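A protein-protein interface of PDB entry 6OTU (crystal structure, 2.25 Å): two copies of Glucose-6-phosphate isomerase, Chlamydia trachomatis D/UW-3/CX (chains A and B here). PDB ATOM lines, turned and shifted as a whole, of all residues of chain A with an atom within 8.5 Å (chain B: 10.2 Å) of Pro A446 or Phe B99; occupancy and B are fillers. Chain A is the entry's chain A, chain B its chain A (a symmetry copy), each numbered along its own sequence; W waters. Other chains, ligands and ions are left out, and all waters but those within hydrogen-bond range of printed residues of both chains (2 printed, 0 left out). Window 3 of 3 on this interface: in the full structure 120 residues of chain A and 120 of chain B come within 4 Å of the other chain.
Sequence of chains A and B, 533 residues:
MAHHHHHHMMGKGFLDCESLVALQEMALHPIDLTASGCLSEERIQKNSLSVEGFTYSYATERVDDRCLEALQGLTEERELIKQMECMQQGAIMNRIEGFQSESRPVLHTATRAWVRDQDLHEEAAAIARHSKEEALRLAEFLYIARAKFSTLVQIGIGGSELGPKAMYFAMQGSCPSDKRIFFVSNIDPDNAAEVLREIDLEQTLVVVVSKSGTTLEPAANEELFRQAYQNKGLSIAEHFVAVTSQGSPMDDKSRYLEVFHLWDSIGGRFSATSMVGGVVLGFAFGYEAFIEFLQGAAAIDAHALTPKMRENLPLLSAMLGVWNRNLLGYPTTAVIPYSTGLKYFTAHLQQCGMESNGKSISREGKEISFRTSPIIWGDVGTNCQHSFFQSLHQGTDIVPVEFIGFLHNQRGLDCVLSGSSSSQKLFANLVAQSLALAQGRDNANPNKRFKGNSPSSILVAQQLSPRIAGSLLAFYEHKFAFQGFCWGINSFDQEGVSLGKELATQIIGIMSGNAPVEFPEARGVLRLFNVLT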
ATOM      1  N   GLN A 394     -19.867 -17.282  -9.234  1.00  0.00           N
ATOM      2  CA  GLN A 394     -19.254 -18.369  -9.996  1.00  0.00           C
ATOM      3  C   GLN A 394     -19.560 -19.764  -9.473  1.00  0.00           C
ATOM      4  O   GLN A 394     -19.074 -20.736 -10.059  1.00  0.00           O
ATOM      5  CB  GLN A 394     -17.722 -18.199 -10.063  1.00  0.00           C
ATOM      6  CG  GLN A 394     -17.239 -17.122 -11.026  1.00  0.00           C
ATOM      7  CD  GLN A 394     -15.752 -17.239 -11.298  1.00  0.00           C
ATOM      8  OE1 GLN A 394     -14.975 -17.540 -10.394  1.00  0.00           O
ATOM      9  NE2 GLN A 394     -15.347 -17.016 -12.549  1.00  0.00           N
ATOM     10  N   ARG A 441     -20.463 -11.379 -17.214  1.00  0.00           N
ATOM     11  CA  ARG A 441     -19.304 -11.017 -18.036  1.00  0.00           C
ATOM     12  C   ARG A 441     -18.810 -12.217 -18.817  1.00  0.00           C
ATOM     13  O   ARG A 441     -18.330 -13.176 -18.210  1.00  0.00           O
ATOM     14  CB  ARG A 441     -18.166 -10.503 -17.186  1.00  0.00           C
ATOM     15  CG  ARG A 441     -18.129  -9.063 -17.247  1.00  0.00           C
ATOM     16  CD  ARG A 441     -17.534  -8.444 -16.011  1.00  0.00           C
ATOM     17  NE  ARG A 441     -17.984  -7.060 -15.999  1.00  0.00           N
ATOM     18  CZ  ARG A 441     -19.235  -6.688 -15.740  1.00  0.00           C
ATOM     19  NH1 ARG A 441     -20.134  -7.638 -15.363  1.00  0.00           N
ATOM     20  NH2 ARG A 441     -19.579  -5.395 -15.819  1.00  0.00           N
ATOM     21  N   ASP A 442     -18.813 -12.126 -20.141  1.00  0.00           N
ATOM     22  CA  ASP A 442     -18.173 -13.168 -20.920  1.00  0.00           C
ATOM     23  C   ASP A 442     -16.655 -13.102 -20.735  1.00  0.00           C
ATOM     24  O   ASP A 442     -16.099 -12.101 -20.264  1.00  0.00           O
ATOM     25  CB  ASP A 442     -18.545 -13.050 -22.398  1.00  0.00           C
ATOM     26  N   ASN A 443     -15.986 -14.206 -21.077  1.00  0.00           N
ATOM     27  CA  ASN A 443     -14.526 -14.252 -21.048  1.00  0.00           C
ATOM     28  C   ASN A 443     -14.046 -15.466 -21.830  1.00  0.00           C
ATOM     29  O   ASN A 443     -14.686 -16.520 -21.795  1.00  0.00           O
ATOM     30  CB  ASN A 443     -13.989 -14.305 -19.608  1.00  0.00           C
ATOM     31  CG  ASN A 443     -12.594 -13.725 -19.491  1.00  0.00           C
ATOM     32  OD1 ASN A 443     -11.613 -14.371 -19.870  1.00  0.00           O
ATOM     33  ND2 ASN A 443     -12.497 -12.502 -18.982  1.00  0.00           N
ATOM     34  N   ALA A 444     -12.920 -15.316 -22.527  1.00  0.00           N
ATOM     35  CA  ALA A 444     -12.328 -16.472 -23.197  1.00  0.00           C
ATOM     36  C   ALA A 444     -11.810 -17.480 -22.184  1.00  0.00           C
ATOM     37  O   ALA A 444     -11.872 -18.691 -22.426  1.00  0.00           O
ATOM     38  CB  ALA A 444     -11.202 -16.033 -24.129  1.00  0.00           C
ATOM     39  N   ASN A 445     -11.306 -16.997 -21.053  1.00  0.00           N
ATOM     40  CA  ASN A 445     -10.859 -17.850 -19.959  1.00  0.00           C
ATOM     41  C   ASN A 445     -12.066 -18.297 -19.134  1.00  0.00           C
ATOM     42  O   ASN A 445     -12.761 -17.445 -18.560  1.00  0.00           O
ATOM     43  CB  ASN A 445      -9.865 -17.072 -19.096  1.00  0.00           C
ATOM     44  CG  ASN A 445      -9.141 -17.937 -18.078  1.00  0.00           C
ATOM     45  OD1 ASN A 445      -9.685 -18.915 -17.566  1.00  0.00           O
ATOM     46  ND2 ASN A 445      -7.908 -17.556 -17.761  1.00  0.00           N
ATOM     47  N   PRO A 446     -12.365 -19.601 -19.061  1.00  0.00           N
ATOM     48  CA  PRO A 446     -13.530 -20.033 -18.271  1.00  0.00           C
ATOM     49  C   PRO A 446     -13.409 -19.693 -16.789  1.00  0.00           C
ATOM     50  O   PRO A 446     -14.431 -19.430 -16.150  1.00  0.00           O
ATOM     51  CB  PRO A 446     -13.583 -21.551 -18.505  1.00  0.00           C
ATOM     52  CG  PRO A 446     -12.708 -21.817 -19.665  1.00  0.00           C
ATOM     53  CD  PRO A 446     -11.660 -20.738 -19.666  1.00  0.00           C
ATOM     54  N   ASN A 447     -12.189 -19.649 -16.232  1.00  0.00           N
ATOM     55  CA  ASN A 447     -12.010 -19.296 -14.827  1.00  0.00           C
ATOM     56  C   ASN A 447     -12.446 -17.862 -14.525  1.00  0.00           C
ATOM     57  O   ASN A 447     -12.680 -17.524 -13.357  1.00  0.00           O
ATOM     58  CB  ASN A 447     -10.546 -19.490 -14.417  1.00  0.00           C
ATOM     59  CG  ASN A 447     -10.393 -19.887 -12.951  1.00  0.00           C
ATOM     60  OD1 ASN A 447     -11.201 -20.639 -12.424  1.00  0.00           O
ATOM     61  ND2 ASN A 447      -9.353 -19.380 -12.291  1.00  0.00           N
ATOM     62  N   LYS A 448     -12.559 -17.016 -15.544  1.00  0.00           N
ATOM     63  CA  LYS A 448     -12.821 -15.597 -15.355  1.00  0.00           C
ATOM     64  C   LYS A 448     -14.157 -15.184 -15.942  1.00  0.00           C
ATOM     65  O   LYS A 448     -14.383 -13.986 -16.151  1.00  0.00           O
ATOM     66  CB  LYS A 448     -11.715 -14.738 -15.982  1.00  0.00           C
ATOM     67  CG  LYS A 448     -10.341 -14.842 -15.355  1.00  0.00           C
ATOM     68  CD  LYS A 448      -9.292 -14.385 -16.381  1.00  0.00           C
ATOM     69  CE  LYS A 448      -8.168 -13.554 -15.770  1.00  0.00           C
ATOM     70  NZ  LYS A 448      -7.219 -14.360 -14.958  1.00  0.00           N
ATOM     71  N   ARG A 449     -15.036 -16.125 -16.252  1.00  0.00           N
ATOM     72  CA  ARG A 449     -16.311 -15.712 -16.796  1.00  0.00           C
ATOM     73  C   ARG A 449     -17.410 -15.826 -15.744  1.00  0.00           C
ATOM     74  O   ARG A 449     -17.323 -16.591 -14.775  1.00  0.00           O
ATOM     75  CB  ARG A 449     -16.665 -16.467 -18.084  1.00  0.00           C
ATOM     76  CG  ARG A 449     -16.800 -17.949 -18.020  1.00  0.00           C
ATOM     77  CD  ARG A 449     -17.322 -18.463 -19.368  1.00  0.00           C
ATOM     78  NE  ARG A 449     -16.286 -18.463 -20.404  1.00  0.00           N
ATOM     79  CZ  ARG A 449     -15.812 -19.560 -20.995  1.00  0.00           C
ATOM     80  NH1 ARG A 449     -16.285 -20.755 -20.655  1.00  0.00           N
ATOM     81  NH2 ARG A 449     -14.865 -19.466 -21.923  1.00  0.00           N
ATOM     82  N   PHE A 450     -18.417 -14.975 -15.920  1.00  0.00           N
ATOM     83  CA  PHE A 450     -19.488 -14.760 -14.960  1.00  0.00           C
ATOM     84  C   PHE A 450     -20.788 -14.854 -15.747  1.00  0.00           C
ATOM     85  O   PHE A 450     -21.025 -14.048 -16.650  1.00  0.00           O
ATOM     86  CB  PHE A 450     -19.315 -13.404 -14.271  1.00  0.00           C
ATOM     87  CG  PHE A 450     -17.973 -13.244 -13.593  1.00  0.00           C
ATOM     88  CD1 PHE A 450     -17.791 -13.646 -12.281  1.00  0.00           C
ATOM     89  CD2 PHE A 450     -16.891 -12.719 -14.275  1.00  0.00           C
ATOM     90  CE1 PHE A 450     -16.549 -13.516 -11.659  1.00  0.00           C
ATOM     91  CE2 PHE A 450     -15.651 -12.580 -13.657  1.00  0.00           C
ATOM     92  CZ  PHE A 450     -15.482 -12.980 -12.354  1.00  0.00           C
ATOM     93  N   LYS A 451     -21.596 -15.878 -15.443  1.00  0.00           N
ATOM     94  CA  LYS A 451     -22.764 -16.192 -16.258  1.00  0.00           C
ATOM     95  C   LYS A 451     -23.883 -15.193 -16.036  1.00  0.00           C
ATOM     96  O   LYS A 451     -24.714 -14.992 -16.930  1.00  0.00           O
ATOM     97  CB  LYS A 451     -23.251 -17.615 -15.956  1.00  0.00           C
ATOM     98  CG  LYS A 451     -22.129 -18.688 -15.996  1.00  0.00           C
ATOM     99  CD  LYS A 451     -22.661 -20.132 -15.786  1.00  0.00           C
ATOM    100  CE  LYS A 451     -21.741 -20.995 -14.891  1.00  0.00           C
ATOM    101  NZ  LYS A 451     -22.097 -20.956 -13.420  1.00  0.00           N
ATOM    102  N   ASN B  94      -2.774 -24.810  -6.856  1.00  0.00           N
ATOM    103  CA  ASN B  94      -3.583 -23.650  -7.227  1.00  0.00           C
ATOM    104  C   ASN B  94      -3.303 -23.359  -8.698  1.00  0.00           C
ATOM    105  O   ASN B  94      -2.436 -22.556  -9.035  1.00  0.00           O
ATOM    106  CB  ASN B  94      -3.241 -22.473  -6.321  1.00  0.00           C
ATOM    107  CG  ASN B  94      -3.983 -21.216  -6.680  1.00  0.00           C
ATOM    108  OD1 ASN B  94      -4.875 -21.228  -7.524  1.00  0.00           O
ATOM    109  ND2 ASN B  94      -3.636 -20.115  -6.015  1.00  0.00           N
ATOM    110  N   ARG B  95      -4.025 -24.030  -9.593  1.00  0.00           N
ATOM    111  CA  ARG B  95      -3.830 -23.753 -11.011  1.00  0.00           C
ATOM    112  C   ARG B  95      -4.970 -24.346 -11.822  1.00  0.00           C
ATOM    113  O   ARG B  95      -5.627 -25.302 -11.406  1.00  0.00           O
ATOM    114  CB  ARG B  95      -2.494 -24.299 -11.515  1.00  0.00           C
ATOM    115  CG  ARG B  95      -2.418 -25.801 -11.568  1.00  0.00           C
ATOM    116  CD  ARG B  95      -1.124 -26.235 -12.257  1.00  0.00           C
ATOM    117  NE  ARG B  95      -1.007 -25.743 -13.631  1.00  0.00           N
ATOM    118  CZ  ARG B  95      -0.935 -26.534 -14.698  1.00  0.00           C
ATOM    119  NH1 ARG B  95      -0.971 -27.853 -14.544  1.00  0.00           N
ATOM    120  NH2 ARG B  95      -0.823 -26.007 -15.917  1.00  0.00           N
ATOM    121  N   ILE B  96      -5.182 -23.766 -13.001  1.00  0.00           N
ATOM    122  CA  ILE B  96      -6.143 -24.255 -13.982  1.00  0.00           C
ATOM    123  C   ILE B  96      -5.363 -24.600 -15.247  1.00  0.00           C
ATOM    124  O   ILE B  96      -4.678 -23.740 -15.815  1.00  0.00           O
ATOM    125  CB  ILE B  96      -7.241 -23.216 -14.277  1.00  0.00           C
ATOM    126  CG1 ILE B  96      -8.074 -22.913 -13.022  1.00  0.00           C
ATOM    127  CG2 ILE B  96      -8.134 -23.693 -15.408  1.00  0.00           C
ATOM    128  CD1 ILE B  96      -8.830 -24.102 -12.483  1.00  0.00           C
ATOM    129  N   GLU B  97      -5.441 -25.860 -15.673  1.00  0.00           N
ATOM    130  CA  GLU B  97      -4.687 -26.285 -16.841  1.00  0.00           C
ATOM    131  C   GLU B  97      -5.361 -25.763 -18.096  1.00  0.00           C
ATOM    132  O   GLU B  97      -6.592 -25.707 -18.183  1.00  0.00           O
ATOM    133  CB  GLU B  97      -4.568 -27.805 -16.898  1.00  0.00           C
ATOM    134  N   GLY B  98      -4.545 -25.351 -19.058  1.00  0.00           N
ATOM    135  CA  GLY B  98      -5.031 -24.868 -20.326  1.00  0.00           C
ATOM    136  C   GLY B  98      -5.244 -23.374 -20.405  1.00  0.00           C
ATOM    137  O   GLY B  98      -5.465 -22.855 -21.509  1.00  0.00           O
ATOM    138  N   PHE B  99      -5.172 -22.665 -19.278  1.00  0.00           N
ATOM    139  CA  PHE B  99      -5.591 -21.272 -19.226  1.00  0.00           C
ATOM    140  C   PHE B  99      -4.699 -20.521 -18.251  1.00  0.00           C
ATOM    141  O   PHE B  99      -3.992 -21.119 -17.434  1.00  0.00           O
ATOM    142  CB  PHE B  99      -7.083 -21.161 -18.829  1.00  0.00           C
ATOM    143  CG  PHE B  99      -8.022 -21.755 -19.856  1.00  0.00           C
ATOM    144  CD1 PHE B  99      -8.377 -21.027 -21.001  1.00  0.00           C
ATOM    145  CD2 PHE B  99      -8.511 -23.055 -19.705  1.00  0.00           C
ATOM    146  CE1 PHE B  99      -9.222 -21.571 -21.968  1.00  0.00           C
ATOM    147  CE2 PHE B  99      -9.349 -23.620 -20.676  1.00  0.00           C
ATOM    148  CZ  PHE B  99      -9.709 -22.870 -21.813  1.00  0.00           C
ATOM    149  N   GLN B 100      -4.730 -19.196 -18.366  1.00  0.00           N
ATOM    150  CA  GLN B 100      -4.078 -18.331 -17.390  1.00  0.00           C
ATOM    151  C   GLN B 100      -4.696 -18.527 -16.007  1.00  0.00           C
ATOM    152  O   GLN B 100      -5.921 -18.562 -15.864  1.00  0.00           O
ATOM    153  CB  GLN B 100      -4.205 -16.871 -17.842  1.00  0.00           C
ATOM    154  CG  GLN B 100      -3.194 -15.913 -17.232  1.00  0.00           C
ATOM    155  CD  GLN B 100      -3.493 -15.624 -15.786  1.00  0.00           C
ATOM    156  OE1 GLN B 100      -4.647 -15.383 -15.414  1.00  0.00           O
ATOM    157  NE2 GLN B 100      -2.462 -15.677 -14.949  1.00  0.00           N
ATOM    158  N   SER B 101      -3.841 -18.654 -14.989  1.00  0.00           N
ATOM    159  CA  SER B 101      -4.260 -18.901 -13.611  1.00  0.00           C
ATOM    160  C   SER B 101      -3.093 -18.531 -12.701  1.00  0.00           C
ATOM    161  O   SER B 101      -1.998 -18.217 -13.177  1.00  0.00           O
ATOM    162  CB  SER B 101      -4.686 -20.359 -13.417  1.00  0.00           C
ATOM    163  OG  SER B 101      -3.646 -21.126 -12.822  1.00  0.00           O
ATOM    164  N   GLU B 102      -3.320 -18.599 -11.379  1.00  0.00           N
ATOM    165  CA  GLU B 102      -2.293 -18.156 -10.433  1.00  0.00           C
ATOM    166  C   GLU B 102      -1.093 -19.109 -10.401  1.00  0.00           C
ATOM    167  O   GLU B 102       0.050 -18.657 -10.234  1.00  0.00           O
ATOM    168  CB  GLU B 102      -2.892 -17.982  -9.034  1.00  0.00           C
ATOM    169  CG  GLU B 102      -4.145 -17.106  -9.016  1.00  0.00           C
ATOM    170  CD  GLU B 102      -4.553 -16.644  -7.619  1.00  0.00           C
ATOM    171  OE1 GLU B 102      -4.200 -17.302  -6.617  1.00  0.00           O
ATOM    172  OE2 GLU B 102      -5.227 -15.606  -7.524  1.00  0.00           O
ATOM    173  N   SER B 103      -1.332 -20.422 -10.531  1.00  0.00           N
ATOM    174  CA  SER B 103      -0.288 -21.441 -10.723  1.00  0.00           C
ATOM    175  C   SER B 103       0.777 -21.397  -9.617  1.00  0.00           C
ATOM    176  O   SER B 103       1.928 -21.036  -9.841  1.00  0.00           O
ATOM    177  CB  SER B 103       0.361 -21.294 -12.106  1.00  0.00           C
ATOM    178  OG  SER B 103       1.129 -22.439 -12.423  1.00  0.00           O
ATOM    179  N   ARG B 104       0.399 -21.829  -8.417  1.00  0.00           N
ATOM    180  CA  ARG B 104       1.340 -21.753  -7.307  1.00  0.00           C
ATOM    181  C   ARG B 104       0.969 -22.800  -6.271  1.00  0.00           C
ATOM    182  O   ARG B 104      -0.115 -23.389  -6.332  1.00  0.00           O
ATOM    183  CB  ARG B 104       1.363 -20.348  -6.690  1.00  0.00           C
ATOM    184  CG  ARG B 104       0.039 -19.827  -6.229  1.00  0.00           C
ATOM    185  CD  ARG B 104       0.058 -18.315  -6.335  1.00  0.00           C
ATOM    186  NE  ARG B 104      -0.891 -17.672  -5.439  1.00  0.00           N
ATOM    187  CZ  ARG B 104      -1.192 -16.376  -5.474  1.00  0.00           C
ATOM    188  NH1 ARG B 104      -0.614 -15.576  -6.363  1.00  0.00           N
ATOM    189  NH2 ARG B 104      -2.081 -15.882  -4.620  1.00  0.00           N
ATOM    190  N   GLY B 358     -16.947 -22.530  -4.176  1.00  0.00           N
ATOM    191  CA  GLY B 358     -17.981 -21.932  -4.999  1.00  0.00           C
ATOM    192  C   GLY B 358     -17.514 -21.770  -6.430  1.00  0.00           C
ATOM    193  O   GLY B 358     -17.300 -20.652  -6.899  1.00  0.00           O
ATOM    194  N   LYS B 359     -17.341 -22.886  -7.131  1.00  0.00           N
ATOM    195  CA  LYS B 359     -16.701 -22.904  -8.438  1.00  0.00           C
ATOM    196  C   LYS B 359     -17.541 -23.727  -9.395  1.00  0.00           C
ATOM    197  O   LYS B 359     -18.334 -24.576  -8.976  1.00  0.00           O
ATOM    198  CB  LYS B 359     -15.291 -23.490  -8.363  1.00  0.00           C
ATOM    199  CG  LYS B 359     -14.411 -22.844  -7.308  1.00  0.00           C
ATOM    200  CD  LYS B 359     -13.987 -21.440  -7.751  1.00  0.00           C
ATOM    201  CE  LYS B 359     -13.331 -20.677  -6.614  1.00  0.00           C
ATOM    202  NZ  LYS B 359     -12.127 -21.376  -6.111  1.00  0.00           N
ATOM    203  N   SER B 360     -17.372 -23.464 -10.691  1.00  0.00           N
ATOM    204  CA  SER B 360     -18.157 -24.201 -11.672  1.00  0.00           C
ATOM    205  C   SER B 360     -17.324 -24.554 -12.902  1.00  0.00           C
ATOM    206  O   SER B 360     -17.875 -24.743 -13.988  1.00  0.00           O
ATOM    207  CB  SER B 360     -19.417 -23.422 -12.067  1.00  0.00           C
ATOM    208  OG  SER B 360     -19.100 -22.073 -12.313  1.00  0.00           O
ATOM    209  N   ILE B 361     -16.000 -24.657 -12.737  1.00  0.00           N
ATOM    210  CA  ILE B 361     -15.096 -25.234 -13.727  1.00  0.00           C
ATOM    211  C   ILE B 361     -14.085 -26.119 -13.002  1.00  0.00           C
ATOM    212  O   ILE B 361     -13.730 -25.864 -11.846  1.00  0.00           O
ATOM    213  CB  ILE B 361     -14.360 -24.160 -14.563  1.00  0.00           C
ATOM    214  CG1 ILE B 361     -13.621 -23.195 -13.644  1.00  0.00           C
ATOM    215  CG2 ILE B 361     -15.318 -23.434 -15.481  1.00  0.00           C
ATOM    216  CD1 ILE B 361     -12.144 -23.383 -13.692  1.00  0.00           C
ATOM    217  N   SER B 362     -13.619 -27.162 -13.700  1.00  0.00           N
ATOM    218  CA  SER B 362     -12.642 -28.120 -13.181  1.00  0.00           C
ATOM    219  C   SER B 362     -11.216 -27.573 -13.283  1.00  0.00           C
ATOM    220  O   SER B 362     -10.934 -26.624 -14.023  1.00  0.00           O
ATOM    221  CB  SER B 362     -12.721 -29.438 -13.959  1.00  0.00           C
ATOM    222  OG  SER B 362     -12.169 -29.310 -15.267  1.00  0.00           O
ATOM    223  N   ARG B 363     -10.292 -28.216 -12.554  1.00  0.00           N
ATOM    224  CA  ARG B 363      -8.872 -27.872 -12.670  1.00  0.00           C
ATOM    225  C   ARG B 363      -8.351 -28.071 -14.086  1.00  0.00           C
ATOM    226  O   ARG B 363      -7.275 -27.560 -14.414  1.00  0.00           O
ATOM    227  CB  ARG B 363      -8.027 -28.694 -11.694  1.00  0.00           C
ATOM    228  CG  ARG B 363      -8.176 -28.277 -10.228  1.00  0.00           C
ATOM    229  CD  ARG B 363      -7.464 -29.235  -9.257  1.00  0.00           C
ATOM    230  NE  ARG B 363      -7.958 -30.611  -9.351  1.00  0.00           N
ATOM    231  CZ  ARG B 363      -7.602 -31.599  -8.535  1.00  0.00           C
ATOM    232  NH1 ARG B 363      -6.746 -31.369  -7.548  1.00  0.00           N
ATOM    233  NH2 ARG B 363      -8.102 -32.821  -8.704  1.00  0.00           N
ATOM    234  N   GLU B 364      -9.087 -28.788 -14.935  1.00  0.00           N
ATOM    235  CA  GLU B 364      -8.754 -28.939 -16.344  1.00  0.00           C
ATOM    236  C   GLU B 364      -9.447 -27.893 -17.236  1.00  0.00           C
ATOM    237  O   GLU B 364      -9.334 -27.960 -18.464  1.00  0.00           O
ATOM    238  CB  GLU B 364      -9.093 -30.368 -16.801  1.00  0.00           C
ATOM    239  N   GLY B 365     -10.146 -26.924 -16.653  1.00  0.00           N
ATOM    240  CA  GLY B 365     -10.783 -25.883 -17.442  1.00  0.00           C
ATOM    241  C   GLY B 365     -12.138 -26.218 -18.035  1.00  0.00           C
ATOM    242  O   GLY B 365     -12.672 -25.411 -18.811  1.00  0.00           O
ATOM    243  N   LYS B 366     -12.714 -27.372 -17.703  1.00  0.00           N
ATOM    244  CA  LYS B 366     -14.004 -27.788 -18.245  1.00  0.00           C
ATOM    245  C   LYS B 366     -15.139 -27.372 -17.316  1.00  0.00           C
ATOM    246  O   LYS B 366     -15.024 -27.474 -16.088  1.00  0.00           O
ATOM    247  CB  LYS B 366     -14.035 -29.303 -18.460  1.00  0.00           C
ATOM    248  N   GLU B 367     -16.227 -26.878 -17.909  1.00  0.00           N
ATOM    249  CA  GLU B 367     -17.434 -26.597 -17.140  1.00  0.00           C
ATOM    250  C   GLU B 367     -17.999 -27.902 -16.583  1.00  0.00           C
ATOM    251  O   GLU B 367     -18.093 -28.900 -17.299  1.00  0.00           O
ATOM    252  CB  GLU B 367     -18.475 -25.885 -18.014  1.00  0.00           C
ATOM    253  N   ILE B 368     -18.372 -27.899 -15.302  1.00  0.00           N
ATOM    254  CA  ILE B 368     -18.799 -29.126 -14.638  1.00  0.00           C
ATOM    255  C   ILE B 368     -20.309 -29.287 -14.760  1.00  0.00           C
ATOM    256  O   ILE B 368     -21.046 -28.336 -15.030  1.00  0.00           O
ATOM    257  CB  ILE B 368     -18.357 -29.150 -13.164  1.00  0.00           C
ATOM    258  CG1 ILE B 368     -18.996 -28.001 -12.409  1.00  0.00           C
ATOM    259  CG2 ILE B 368     -16.816 -29.116 -13.049  1.00  0.00           C
ATOM    260  CD1 ILE B 368     -18.562 -27.920 -10.982  1.00  0.00           C
ATOM    261  N   ASN B 490     -10.605 -26.151  -8.420  1.00  0.00           N
ATOM    262  CA  ASN B 490      -9.503 -25.434  -7.778  1.00  0.00           C
ATOM    263  C   ASN B 490     -10.060 -24.700  -6.563  1.00  0.00           C
ATOM    264  O   ASN B 490     -10.708 -23.651  -6.686  1.00  0.00           O
ATOM    265  CB  ASN B 490      -8.803 -24.490  -8.750  1.00  0.00           C
ATOM    266  CG  ASN B 490      -7.666 -23.694  -8.086  1.00  0.00           C
ATOM    267  OD1 ASN B 490      -7.294 -23.962  -6.943  1.00  0.00           O
ATOM    268  ND2 ASN B 490      -7.122 -22.698  -8.808  1.00  0.00           N
ATOM    269  N   ASP B 493      -8.148 -20.485  -5.544  1.00  0.00           N
ATOM    270  CA  ASP B 493      -8.217 -19.131  -6.083  1.00  0.00           C
ATOM    271  C   ASP B 493      -9.625 -18.568  -5.875  1.00  0.00           C
ATOM    272  O   ASP B 493     -10.480 -19.176  -5.212  1.00  0.00           O
ATOM    273  CB  ASP B 493      -7.769 -19.096  -7.557  1.00  0.00           C
ATOM    274  CG  ASP B 493      -8.641 -19.946  -8.466  1.00  0.00           C
ATOM    275  OD1 ASP B 493      -9.559 -20.644  -7.952  1.00  0.00           O
ATOM    276  OD2 ASP B 493      -8.390 -19.914  -9.697  1.00  0.00           O
ATOM    277  N   GLU B 495     -11.570 -15.969  -8.402  1.00  0.00           N
ATOM    278  CA  GLU B 495     -11.747 -14.980  -9.458  1.00  0.00           C
ATOM    279  C   GLU B 495     -12.990 -14.120  -9.245  1.00  0.00           C
ATOM    280  O   GLU B 495     -13.043 -12.995  -9.760  1.00  0.00           O
ATOM    281  CB  GLU B 495     -11.788 -15.682 -10.808  1.00  0.00           C
ATOM    282  CG  GLU B 495     -10.426 -16.200 -11.240  1.00  0.00           C
ATOM    283  CD  GLU B 495      -9.384 -15.091 -11.383  1.00  0.00           C
ATOM    284  OE1 GLU B 495      -9.728 -13.988 -11.884  1.00  0.00           O
ATOM    285  OE2 GLU B 495      -8.222 -15.322 -10.976  1.00  0.00           O
ATOM    286  N   GLY B 496     -13.986 -14.615  -8.499  1.00  0.00           N
ATOM    287  CA  GLY B 496     -15.124 -13.777  -8.137  1.00  0.00           C
ATOM    288  C   GLY B 496     -14.744 -12.635  -7.211  1.00  0.00           C
ATOM    289  O   GLY B 496     -15.265 -11.521  -7.341  1.00  0.00           O
HETATM  290  O   HOH W   1      -7.728 -17.594 -13.794  1.00  0.00           O
HETATM  291  O   HOH W   2      -6.174 -17.695 -20.198  1.00  0.00           O
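O of Gln A394 is in hydrogen-bond range of OG of Ser B360 (2.6 Å). The side-chain amide nitrogen of Asn A445 sits at hydrogen-bond distance from the backbone carbonyl oxygen of Gln B100. The side-chain amide nitrogen (ND2) of Asn A447 sits at hydrogen-bond distance from the side-chain carboxylate (OD2) of Asp B493. OE1 of Gln B100 is in hydrogen-bond range of NZ of Lys A448, 2.8 Å away. The side-chain amino group (NZ) of Lys A448 lies within salt-bridge range of the side-chain carboxylate (OE1) of Glu B495, 3.99 Å away. NZ of Lys A451 sits at hydrogen-bond distance from OG of Ser B360, at 3.4 Å.
The side-chain amide nitrogen of Gln A394 lies within hydrogen-bond range of the backbone carbonyl oxygen of Arg A449 (3.0 Å). N of Arg A441 is in hydrogen-bond range of O of Phe A450 (2.8 Å). NH2 of Arg A449 is in hydrogen-bond range of O of Ala A444. The side-chain amino group (NZ) of Lys B359 lies within hydrogen-bond range of the backbone carbonyl oxygen (O) of Asn B490 (2.7 Å). O of Ser B360 lies within hydrogen-bond range of N of Ile B368 (3.5 Å). The backbone NH (N) of Gly B365 lies within hydrogen-bond range of the side-chain hydroxyl (OG) of Ser B362.
C of Gln A394 touches O of Gly B358 (3.5 Å). Lys B359 touches Gln A394 (C to O, 3.4 Å). Glu B495 touches Gln A394. CB of Phe B99 touches OD1 of Asn A445 (3.7 Å). Pro A446 touches Phe B99 (CD to CE1, 3.5 Å). Pro A446 touches Ile B361 (CB to CG2, 3.96 Å). Asn A447 touches Ile B361 (OD1 to CD1, 3.2 Å). O of Asn A447 touches CB of Glu B495, at 3.3 Å. Phe A450 touches Glu B495 (CZ to O, 3.6 Å). Gly B496 touches Phe A450.
Of the printed residues of chain B, Pro A446 touches Phe B99, Ile B361 and Gly B365. Of chain A, only Ala A444, Asn A445 and Pro A446 come within 4 Å of Phe B99. Printed residues of chain B within 4 Å of Asn A447: Ile B96 (3.8 Å), Ile B361 (3.2 Å), Asp B493 (2.8 Å) and Glu B495 (3.3 Å). No residue of chain B comes within 4 Å of Arg A449. Gly B98 touches none of the printed residues of chain A. Of the printed residues of chain A, Asp B493 touches Asn A447. Printed residues of chain A within 4 Å of Glu B495: Gln A394 (3.7 Å), Asn A447 (3.3 Å), Lys A448 (3.6 Å) and Phe A450 (3.6 Å). Printed residues of chain B within 4 Å of Lys A451: Ser B360. Printed residues of chain A within 4 Å of Lys B359: Gln A394. Of the printed residues of chain B, Ala A444 touches Phe B99. Asn B94 touches none of the printed residues of chain A. Asn A443 touches none of the printed residues of chain B. The nearest residue of chain B that does not touch Pro A446 is Lys B366 (5.9 Å).
Hydrophobic or aromatic side chains of chain B that line the printed part of chain A: Ile B96, Phe B99 and Ile B361. Of the 12 printed residues of chain A, 8 touch a printed residue of chain B.
No position is printed for both chains. Of the 20 pairs that touch across the chains among the printed residues, none has its exchanged pair printed and touching as well.
Water W2 bridges the backbone NH of Gln B100 and the side-chain amide nitrogen of Asn A445. Water W1 lies within hydrogen-bond range of ND2 of Asn A447 (2.8 Å), O of Gln B100 (2.9 Å) and NZ of Lys A448 (3.5 Å).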
